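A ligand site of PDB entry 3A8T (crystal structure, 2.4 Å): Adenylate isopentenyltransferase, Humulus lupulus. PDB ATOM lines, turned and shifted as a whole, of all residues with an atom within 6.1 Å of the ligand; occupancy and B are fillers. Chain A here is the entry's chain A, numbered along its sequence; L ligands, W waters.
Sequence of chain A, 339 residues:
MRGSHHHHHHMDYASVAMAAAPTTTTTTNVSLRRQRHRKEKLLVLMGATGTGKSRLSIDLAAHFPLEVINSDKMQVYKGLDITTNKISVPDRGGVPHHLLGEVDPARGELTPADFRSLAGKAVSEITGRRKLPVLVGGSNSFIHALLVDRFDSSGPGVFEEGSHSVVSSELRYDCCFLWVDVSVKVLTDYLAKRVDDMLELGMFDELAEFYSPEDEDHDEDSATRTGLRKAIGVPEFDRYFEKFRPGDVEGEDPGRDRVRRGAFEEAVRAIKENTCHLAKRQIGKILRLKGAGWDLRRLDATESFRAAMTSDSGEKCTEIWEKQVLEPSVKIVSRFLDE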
ATOM      1  N   THR A  49      16.864   5.297   0.387  1.00  0.00           N
ATOM      2  CA  THR A  49      15.629   5.167   1.147  1.00  0.00           C
ATOM      3  C   THR A  49      15.767   5.735   2.546  1.00  0.00           C
ATOM      4  O   THR A  49      16.743   5.458   3.248  1.00  0.00           O
ATOM      5  CB  THR A  49      15.254   3.687   1.274  1.00  0.00           C
ATOM      6  OG1 THR A  49      14.202   3.525   2.230  1.00  0.00           O
ATOM      7  CG2 THR A  49      16.490   2.868   1.704  1.00  0.00           C
ATOM      8  N   SER A  71       8.920   9.547  -7.375  1.00  0.00           N
ATOM      9  CA  SER A  71       9.756   8.684  -8.236  1.00  0.00           C
ATOM     10  C   SER A  71      10.126   7.361  -7.555  1.00  0.00           C
ATOM     11  O   SER A  71      10.988   6.625  -8.027  1.00  0.00           O
ATOM     12  CB  SER A  71      11.038   9.401  -8.664  1.00  0.00           C
ATOM     13  OG  SER A  71      11.781   9.802  -7.546  1.00  0.00           O
ATOM     14  N   ASP A  72       9.493   7.064  -6.433  1.00  0.00           N
ATOM     15  CA  ASP A  72       9.725   5.805  -5.726  1.00  0.00           C
ATOM     16  C   ASP A  72       8.753   4.792  -6.388  1.00  0.00           C
ATOM     17  O   ASP A  72       7.546   4.977  -6.447  1.00  0.00           O
ATOM     18  CB  ASP A  72       9.460   6.031  -4.254  1.00  0.00           C
ATOM     19  CG  ASP A  72       9.532   4.782  -3.450  1.00  0.00           C
ATOM     20  OD1 ASP A  72       8.788   3.829  -3.742  1.00  0.00           O
ATOM     21  OD2 ASP A  72      10.343   4.752  -2.495  1.00  0.00           O
ATOM     22  N   LYS A  73       9.287   3.725  -6.954  1.00  0.00           N
ATOM     23  CA  LYS A  73       8.437   2.792  -7.668  1.00  0.00           C
ATOM     24  C   LYS A  73       7.432   1.943  -6.875  1.00  0.00           C
ATOM     25  O   LYS A  73       6.500   1.382  -7.462  1.00  0.00           O
ATOM     26  CB  LYS A  73       9.295   1.909  -8.611  1.00  0.00           C
ATOM     27  CG  LYS A  73      10.088   0.805  -7.940  1.00  0.00           C
ATOM     28  CD  LYS A  73      10.821  -0.026  -9.017  1.00  0.00           C
ATOM     29  CE  LYS A  73      11.232  -1.405  -8.474  1.00  0.00           C
ATOM     30  NZ  LYS A  73      11.925  -2.242  -9.450  1.00  0.00           N
ATOM     31  N   MET A  74       7.602   1.839  -5.551  1.00  0.00           N
ATOM     32  CA  MET A  74       6.633   1.098  -4.749  1.00  0.00           C
ATOM     33  C   MET A  74       5.507   2.085  -4.339  1.00  0.00           C
ATOM     34  O   MET A  74       4.330   1.727  -4.286  1.00  0.00           O
ATOM     35  CB  MET A  74       7.288   0.496  -3.488  1.00  0.00           C
ATOM     36  CG  MET A  74       8.145  -0.752  -3.763  1.00  0.00           C
ATOM     37  SD  MET A  74       7.128  -2.076  -4.588  1.00  0.00           S
ATOM     38  CE  MET A  74       7.794  -1.988  -6.209  1.00  0.00           C
ATOM     39  N   GLN A  75       5.888   3.333  -4.090  1.00  0.00           N
ATOM     40  CA  GLN A  75       4.974   4.365  -3.659  1.00  0.00           C
ATOM     41  C   GLN A  75       3.968   4.821  -4.696  1.00  0.00           C
ATOM     42  O   GLN A  75       3.091   5.624  -4.373  1.00  0.00           O
ATOM     43  CB  GLN A  75       5.755   5.574  -3.135  1.00  0.00           C
ATOM     44  CG  GLN A  75       6.450   5.283  -1.832  1.00  0.00           C
ATOM     45  CD  GLN A  75       6.972   6.497  -1.141  1.00  0.00           C
ATOM     46  OE1 GLN A  75       6.776   7.620  -1.573  1.00  0.00           O
ATOM     47  NE2 GLN A  75       7.653   6.287  -0.058  1.00  0.00           N
ATOM     48  N   THR A  83       3.893   0.353   5.094  1.00  0.00           N
ATOM     49  CA  THR A  83       4.974  -0.471   4.590  1.00  0.00           C
ATOM     50  C   THR A  83       5.834   0.239   3.542  1.00  0.00           C
ATOM     51  O   THR A  83       7.048   0.069   3.554  1.00  0.00           O
ATOM     52  CB  THR A  83       4.434  -1.838   4.003  1.00  0.00           C
ATOM     53  OG1 THR A  83       3.654  -2.537   5.005  1.00  0.00           O
ATOM     54  CG2 THR A  83       5.627  -2.743   3.601  1.00  0.00           C
ATOM     55  N   THR A  84       5.214   1.047   2.690  1.00  0.00           N
ATOM     56  CA  THR A  84       5.952   1.727   1.644  1.00  0.00           C
ATOM     57  C   THR A  84       6.561   3.046   2.021  1.00  0.00           C
ATOM     58  O   THR A  84       7.306   3.631   1.241  1.00  0.00           O
ATOM     59  CB  THR A  84       5.109   1.932   0.307  1.00  0.00           C
ATOM     60  OG1 THR A  84       3.875   2.571   0.600  1.00  0.00           O
ATOM     61  CG2 THR A  84       4.869   0.578  -0.402  1.00  0.00           C
ATOM     62  N   ASN A  85       6.256   3.485   3.251  1.00  0.00           N
ATOM     63  CA  ASN A  85       6.745   4.701   3.837  1.00  0.00           C
ATOM     64  C   ASN A  85       6.245   5.925   3.080  1.00  0.00           C
ATOM     65  O   ASN A  85       7.034   6.851   2.810  1.00  0.00           O
ATOM     66  CB  ASN A  85       8.271   4.675   3.899  1.00  0.00           C
ATOM     67  CG  ASN A  85       8.849   3.282   4.382  1.00  0.00           C
ATOM     68  OD1 ASN A  85       9.322   2.434   3.538  1.00  0.00           O
ATOM     69  ND2 ASN A  85       8.821   3.049   5.700  1.00  0.00           N
ATOM     70  N   GLY A 138      13.601   7.472  -4.832  1.00  0.00           N
ATOM     71  CA  GLY A 138      14.816   6.748  -4.998  1.00  0.00           C
ATOM     72  C   GLY A 138      14.911   5.617  -5.980  1.00  0.00           C
ATOM     73  O   GLY A 138      15.868   4.835  -5.859  1.00  0.00           O
ATOM     74  N   SER A 139      13.978   5.495  -6.923  1.00  0.00           N
ATOM     75  CA  SER A 139      14.103   4.413  -7.910  1.00  0.00           C
ATOM     76  C   SER A 139      14.846   4.991  -9.067  1.00  0.00           C
ATOM     77  O   SER A 139      14.280   5.671  -9.924  1.00  0.00           O
ATOM     78  CB  SER A 139      12.766   3.893  -8.374  1.00  0.00           C
ATOM     79  OG  SER A 139      12.033   3.483  -7.241  1.00  0.00           O
ATOM     80  N   ASN A 140      16.141   4.751  -9.056  1.00  0.00           N
ATOM     81  CA  ASN A 140      17.021   5.265 -10.081  1.00  0.00           C
ATOM     82  C   ASN A 140      16.570   4.786 -11.458  1.00  0.00           C
ATOM     83  O   ASN A 140      16.782   5.482 -12.423  1.00  0.00           O
ATOM     84  CB  ASN A 140      18.474   4.948  -9.702  1.00  0.00           C
ATOM     85  CG  ASN A 140      18.906   5.714  -8.391  1.00  0.00           C
ATOM     86  OD1 ASN A 140      18.897   6.962  -8.340  1.00  0.00           O
ATOM     87  ND2 ASN A 140      19.278   4.958  -7.326  1.00  0.00           N
ATOM     88  N   SER A 141      15.881   3.658 -11.531  1.00  0.00           N
ATOM     89  CA  SER A 141      15.366   3.201 -12.812  1.00  0.00           C
ATOM     90  C   SER A 141      14.214   4.127 -13.286  1.00  0.00           C
ATOM     91  O   SER A 141      14.029   4.317 -14.513  1.00  0.00           O
ATOM     92  CB  SER A 141      14.860   1.763 -12.727  1.00  0.00           C
ATOM     93  OG  SER A 141      13.553   1.665 -12.137  1.00  0.00           O
ATOM     94  N   PHE A 142      13.435   4.677 -12.367  1.00  0.00           N
ATOM     95  CA  PHE A 142      12.349   5.583 -12.733  1.00  0.00           C
ATOM     96  C   PHE A 142      12.907   6.962 -13.018  1.00  0.00           C
ATOM     97  O   PHE A 142      12.484   7.616 -13.948  1.00  0.00           O
ATOM     98  CB  PHE A 142      11.262   5.664 -11.649  1.00  0.00           C
ATOM     99  CG  PHE A 142      10.165   4.605 -11.769  1.00  0.00           C
ATOM    100  CD1 PHE A 142      10.345   3.465 -12.565  1.00  0.00           C
ATOM    101  CD2 PHE A 142       8.945   4.756 -11.113  1.00  0.00           C
ATOM    102  CE1 PHE A 142       9.320   2.515 -12.698  1.00  0.00           C
ATOM    103  CE2 PHE A 142       7.941   3.800 -11.241  1.00  0.00           C
ATOM    104  CZ  PHE A 142       8.134   2.693 -12.047  1.00  0.00           C
ATOM    105  N   SER A 222      11.595 -10.541  -3.319  1.00  0.00           N
ATOM    106  CA  SER A 222      11.204  -9.245  -3.883  1.00  0.00           C
ATOM    107  C   SER A 222      11.758  -9.100  -5.323  1.00  0.00           C
ATOM    108  O   SER A 222      11.084  -8.565  -6.196  1.00  0.00           O
ATOM    109  CB  SER A 222      11.839  -8.107  -3.074  1.00  0.00           C
ATOM    110  OG  SER A 222      11.137  -7.809  -1.881  1.00  0.00           O
ATOM    111  N   ALA A 223      12.975  -9.584  -5.526  1.00  0.00           N
ATOM    112  CA  ALA A 223      13.692  -9.419  -6.782  1.00  0.00           C
ATOM    113  C   ALA A 223      12.901  -9.791  -7.988  1.00  0.00           C
ATOM    114  O   ALA A 223      12.934  -9.081  -8.976  1.00  0.00           O
ATOM    115  CB  ALA A 223      14.996 -10.209  -6.751  1.00  0.00           C
ATOM    116  N   GLY A 227       5.375  -5.897  -9.018  1.00  0.00           N
ATOM    117  CA  GLY A 227       4.694  -4.722  -8.486  1.00  0.00           C
ATOM    118  C   GLY A 227       4.808  -4.482  -6.969  1.00  0.00           C
ATOM    119  O   GLY A 227       5.886  -4.736  -6.362  1.00  0.00           O
ATOM    120  N   LYS A 230       6.564  -6.563  -4.373  1.00  0.00           N
ATOM    121  CA  LYS A 230       8.008  -6.505  -4.223  1.00  0.00           C
ATOM    122  C   LYS A 230       8.468  -5.690  -2.977  1.00  0.00           C
ATOM    123  O   LYS A 230       9.592  -5.861  -2.541  1.00  0.00           O
ATOM    124  CB  LYS A 230       8.671  -5.811  -5.417  1.00  0.00           C
ATOM    125  CG  LYS A 230       8.496  -6.520  -6.732  1.00  0.00           C
ATOM    126  CD  LYS A 230       9.168  -5.722  -7.829  1.00  0.00           C
ATOM    127  CE  LYS A 230      10.547  -6.256  -8.074  1.00  0.00           C
ATOM    128  NZ  LYS A 230      11.298  -5.354  -8.991  1.00  0.00           N
ATOM    129  N   ALA A 231       7.603  -4.833  -2.448  1.00  0.00           N
ATOM    130  CA  ALA A 231       7.884  -3.955  -1.304  1.00  0.00           C
ATOM    131  C   ALA A 231       8.580  -4.651  -0.171  1.00  0.00           C
ATOM    132  O   ALA A 231       8.166  -5.749   0.184  1.00  0.00           O
ATOM    133  CB  ALA A 231       6.588  -3.339  -0.818  1.00  0.00           C
ATOM    134  N   ILE A 232       9.641  -4.059   0.407  1.00  0.00           N
ATOM    135  CA  ILE A 232      10.308  -4.754   1.524  1.00  0.00           C
ATOM    136  C   ILE A 232       9.274  -4.892   2.646  1.00  0.00           C
ATOM    137  O   ILE A 232       8.565  -3.932   2.976  1.00  0.00           O
ATOM    138  CB  ILE A 232      11.557  -4.007   2.102  1.00  0.00           C
ATOM    139  CG1 ILE A 232      12.624  -3.748   1.046  1.00  0.00           C
ATOM    140  CG2 ILE A 232      12.193  -4.851   3.167  1.00  0.00           C
ATOM    141  CD1 ILE A 232      13.086  -4.919   0.419  1.00  0.00           C
ATOM    142  N   GLY A 233       9.171  -6.100   3.220  1.00  0.00           N
ATOM    143  CA  GLY A 233       8.184  -6.349   4.260  1.00  0.00           C
ATOM    144  C   GLY A 233       7.182  -7.371   3.795  1.00  0.00           C
ATOM    145  O   GLY A 233       6.755  -8.280   4.539  1.00  0.00           O
ATOM    146  N   LEU A 278      19.322  -2.657   0.505  1.00  0.00           N
ATOM    147  CA  LEU A 278      18.750  -1.820  -0.552  1.00  0.00           C
ATOM    148  C   LEU A 278      19.436  -0.449  -0.491  1.00  0.00           C
ATOM    149  O   LEU A 278      19.750   0.158  -1.508  1.00  0.00           O
ATOM    150  CB  LEU A 278      17.232  -1.659  -0.358  1.00  0.00           C
ATOM    151  CG  LEU A 278      16.605  -0.608  -1.283  1.00  0.00           C
ATOM    152  CD1 LEU A 278      16.781  -1.032  -2.758  1.00  0.00           C
ATOM    153  CD2 LEU A 278      15.140  -0.392  -0.940  1.00  0.00           C
ATOM    154  N   ARG A 281      22.774  -0.604  -2.230  1.00  0.00           N
ATOM    155  CA  ARG A 281      22.710  -0.667  -3.698  1.00  0.00           C
ATOM    156  C   ARG A 281      22.294   0.667  -4.324  1.00  0.00           C
ATOM    157  O   ARG A 281      22.678   0.982  -5.440  1.00  0.00           O
ATOM    158  CB  ARG A 281      21.744  -1.760  -4.164  1.00  0.00           C
ATOM    159  CG  ARG A 281      22.254  -3.139  -3.866  1.00  0.00           C
ATOM    160  CD  ARG A 281      21.376  -4.238  -4.459  1.00  0.00           C
ATOM    161  NE  ARG A 281      20.009  -4.295  -3.924  1.00  0.00           N
ATOM    162  CZ  ARG A 281      19.607  -5.062  -2.891  1.00  0.00           C
ATOM    163  NH1 ARG A 281      20.459  -5.861  -2.232  1.00  0.00           N
ATOM    164  NH2 ARG A 281      18.324  -5.057  -2.549  1.00  0.00           N
ATOM    165  N   GLN A 282      21.493   1.442  -3.598  1.00  0.00           N
ATOM    166  CA  GLN A 282      21.041   2.738  -4.066  1.00  0.00           C
ATOM    167  C   GLN A 282      22.158   3.751  -4.103  1.00  0.00           C
ATOM    168  O   GLN A 282      22.300   4.466  -5.079  1.00  0.00           O
ATOM    169  CB  GLN A 282      19.935   3.242  -3.157  1.00  0.00           C
ATOM    170  CG  GLN A 282      18.634   2.495  -3.399  1.00  0.00           C
ATOM    171  CD  GLN A 282      17.516   2.974  -2.507  1.00  0.00           C
ATOM    172  OE1 GLN A 282      17.715   3.160  -1.314  1.00  0.00           O
ATOM    173  NE2 GLN A 282      16.319   3.168  -3.086  1.00  0.00           N
ATOM    174  N   LYS A 285      24.661   2.973  -6.769  1.00  0.00           N
ATOM    175  CA  LYS A 285      23.994   3.358  -7.986  1.00  0.00           C
ATOM    176  C   LYS A 285      24.091   4.891  -8.132  1.00  0.00           C
ATOM    177  O   LYS A 285      24.425   5.429  -9.209  1.00  0.00           O
ATOM    178  CB  LYS A 285      22.567   2.876  -7.833  1.00  0.00           C
ATOM    179  CG  LYS A 285      21.659   2.909  -9.044  1.00  0.00           C
ATOM    180  CD  LYS A 285      20.429   2.073  -8.739  1.00  0.00           C
ATOM    181  CE  LYS A 285      20.843   0.619  -8.476  1.00  0.00           C
ATOM    182  NZ  LYS A 285      19.707  -0.341  -8.609  1.00  0.00           N
HETATM  183  P1  LIG L   1      15.811  -2.274  -9.259  1.00  0.00           P
HETATM  184  O1  LIG L   1      15.480  -1.943 -10.673  1.00  0.00           O
HETATM  185  O2  LIG L   1      14.754  -3.408  -8.760  1.00  0.00           O
HETATM  186  O3  LIG L   1      17.302  -2.864  -9.139  1.00  0.00           O
HETATM  187  P2  LIG L   1      15.158   0.385  -8.907  1.00  0.00           P
HETATM  188  O4  LIG L   1      16.179   1.257  -9.407  1.00  0.00           O
HETATM  189  O5  LIG L   1      14.229   0.004 -10.097  1.00  0.00           O
HETATM  190  O6  LIG L   1      15.772  -0.932  -8.262  1.00  0.00           O
HETATM  191  P3  LIG L   1      14.488   0.953  -6.234  1.00  0.00           P
HETATM  192  O7  LIG L   1      15.873   0.830  -5.812  1.00  0.00           O
HETATM  193  O8  LIG L   1      13.878   2.253  -5.454  1.00  0.00           O
HETATM  194  O9  LIG L   1      14.267   1.222  -7.846  1.00  0.00           O
HETATM  195  O10 LIG L   1      13.559  -0.273  -5.704  1.00  0.00           O
HETATM  196  C1  LIG L   1      14.177  -1.526  -5.823  1.00  0.00           C
HETATM  197  C2  LIG L   1      13.482  -2.454  -4.839  1.00  0.00           C
HETATM  198  O11 LIG L   1      13.625  -1.911  -3.523  1.00  0.00           O
HETATM  199  C3  LIG L   1      11.951  -2.572  -5.041  1.00  0.00           C
HETATM  200  O12 LIG L   1      11.635  -3.600  -5.984  1.00  0.00           O
HETATM  201  C4  LIG L   1      11.446  -2.873  -3.617  1.00  0.00           C
HETATM  202  O13 LIG L   1      11.524  -4.235  -3.354  1.00  0.00           O
HETATM  203  C5  LIG L   1      12.393  -2.113  -2.713  1.00  0.00           C
HETATM  204  N1  LIG L   1      11.805  -0.804  -2.312  1.00  0.00           N
HETATM  205  C6  LIG L   1      12.034   0.430  -2.910  1.00  0.00           C
HETATM  206  N2  LIG L   1      11.270   1.359  -2.369  1.00  0.00           N
HETATM  207  C7  LIG L   1      10.499   0.787  -1.398  1.00  0.00           C
HETATM  208  C8  LIG L   1       9.478   1.243  -0.466  1.00  0.00           C
HETATM  209  N3  LIG L   1       9.055   2.545  -0.414  1.00  0.00           N
HETATM  210  N4  LIG L   1       8.947   0.333   0.372  1.00  0.00           N
HETATM  211  C9  LIG L   1       9.329  -0.934   0.369  1.00  0.00           C
HETATM  212  N5  LIG L   1      10.256  -1.402  -0.472  1.00  0.00           N
HETATM  213  C10 LIG L   1      10.857  -0.614  -1.343  1.00  0.00           C
HETATM  214  O   HOH W   1      13.190  -5.627  -7.035  1.00  0.00           O
HETATM  215  O   HOH W   2      18.209  -0.441  -5.944  1.00  0.00           O
HETATM  216  O   HOH W   3      17.568   2.825  -7.319  1.00  0.00           O
HETATM  217  O   HOH W   4      17.545  -0.793 -12.883  1.00  0.00           O
HETATM  218  O   HOH W   5      16.711  -4.264  -5.987  1.00  0.00           O
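O of Lys 230 sits at hydrogen-bond distance from OG of Ser 222.
The backbone NH (N) of Ser 139 sits close to the backbone carbonyl oxygen (O) of Ser 71 (3.4 Å).
The side-chain hydroxyl (OG) of Ser 139 is in hydrogen-bond range of the backbone NH (N) of Lys 73 (2.8 Å).
The side-chain amide nitrogen (NE2) of Gln 75 lies within hydrogen-bond range of the backbone carbonyl oxygen (O) of Thr 84.
O of Thr 83 lies close to OD1 of Asn 85, 3.3 Å away.
The backbone carbonyl oxygen (O) of Asn 85 sits at hydrogen-bond distance from the side-chain amide nitrogen (NE2) of Gln 75 (3.0 Å).
NE2 of Gln 282 is in hydrogen-bond range of O of Gly 138, at 3.3 Å.
N of Gln 75 is in hydrogen-bond range of OD1 of Asp 72, at 3.0 Å.
Water W2 lies within hydrogen-bond range of O7 of the ligand (2.7 Å) and NZ of Lys 285 (3.1 Å).
Water W1 lies within hydrogen-bond range of the side-chain amino group of Lys 230 (2.7 Å) and an oxygen (O12) of the ligand (2.8 Å).
Water W3 lies within hydrogen-bond range of ND2 of Asn 140, O4 of the ligand and O of Gly 138.
An oxygen (O8) of the ligand sits close to the backbone carbonyl oxygen (O) of Gly 138, at 3.3 Å.
Met 74 touches the ligand.
Thr 83 touches the ligand.
Asn 85 touches the ligand (OD1 to N4, 3.8 Å).
N of Asn 140 touches O4 of the ligand, 3.5 Å away.
Ser 222 touches the ligand (OG to O13, 3.9 Å).
Ala 231 touches the ligand.
Leu 278 touches the ligand (CD2 to O11, 3.4 Å).
Gln 282 touches the ligand (NE2 to O8, 3.5 Å).
Hydrophobic or aromatic side chains within 4 Å of the ligand: Met 74, Ala 231, Ile 232 and Leu 278.
Within 4 Å of the ligand: Asp 72, Lys 73, Met 74, Thr 83, Thr 84, Asn 85, Gly 138, Ser 139, Asn 140, Ser 141, Ser 222, Lys 230, Ala 231, Ile 232, Leu 278, Gln 282 and Lys 285.
OD2 of Asp 72 lies within hydrogen-bond range of N3 of the ligand (3.3 Å).
The backbone NH of Ser 141 sits at hydrogen-bond distance from an oxygen (O4) of the ligand, 3.2 Å away.
An oxygen (O8) of the ligand is in hydrogen-bond range of the side-chain hydroxyl (OG) of Ser 139, at 2.8 Å.
The backbone NH (N) of Ile 232 sits at hydrogen-bond distance from a nitrogen (N5) of the ligand (2.9 Å).
An oxygen (O3) of the ligand is in salt-bridge range of the side-chain amino group (NZ) of Lys 285 (3.5 Å).
The side-chain amino group (NZ) of Lys 73 is in salt-bridge range of an oxygen (O2) of the ligand (3.1 Å).
O of Lys 230 is in hydrogen-bond range of O13 of the ligand (2.7 Å).
OG of Ser 141 is in hydrogen-bond range of O5 of the ligand (2.7 Å).
An oxygen (O2) of the ligand lies within salt-bridge range of the side-chain amino group (NZ) of Lys 230 (3.97 Å).
The backbone carbonyl oxygen of Thr 84 sits at hydrogen-bond distance from a nitrogen (N3) of the ligand, at 2.6 Å.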
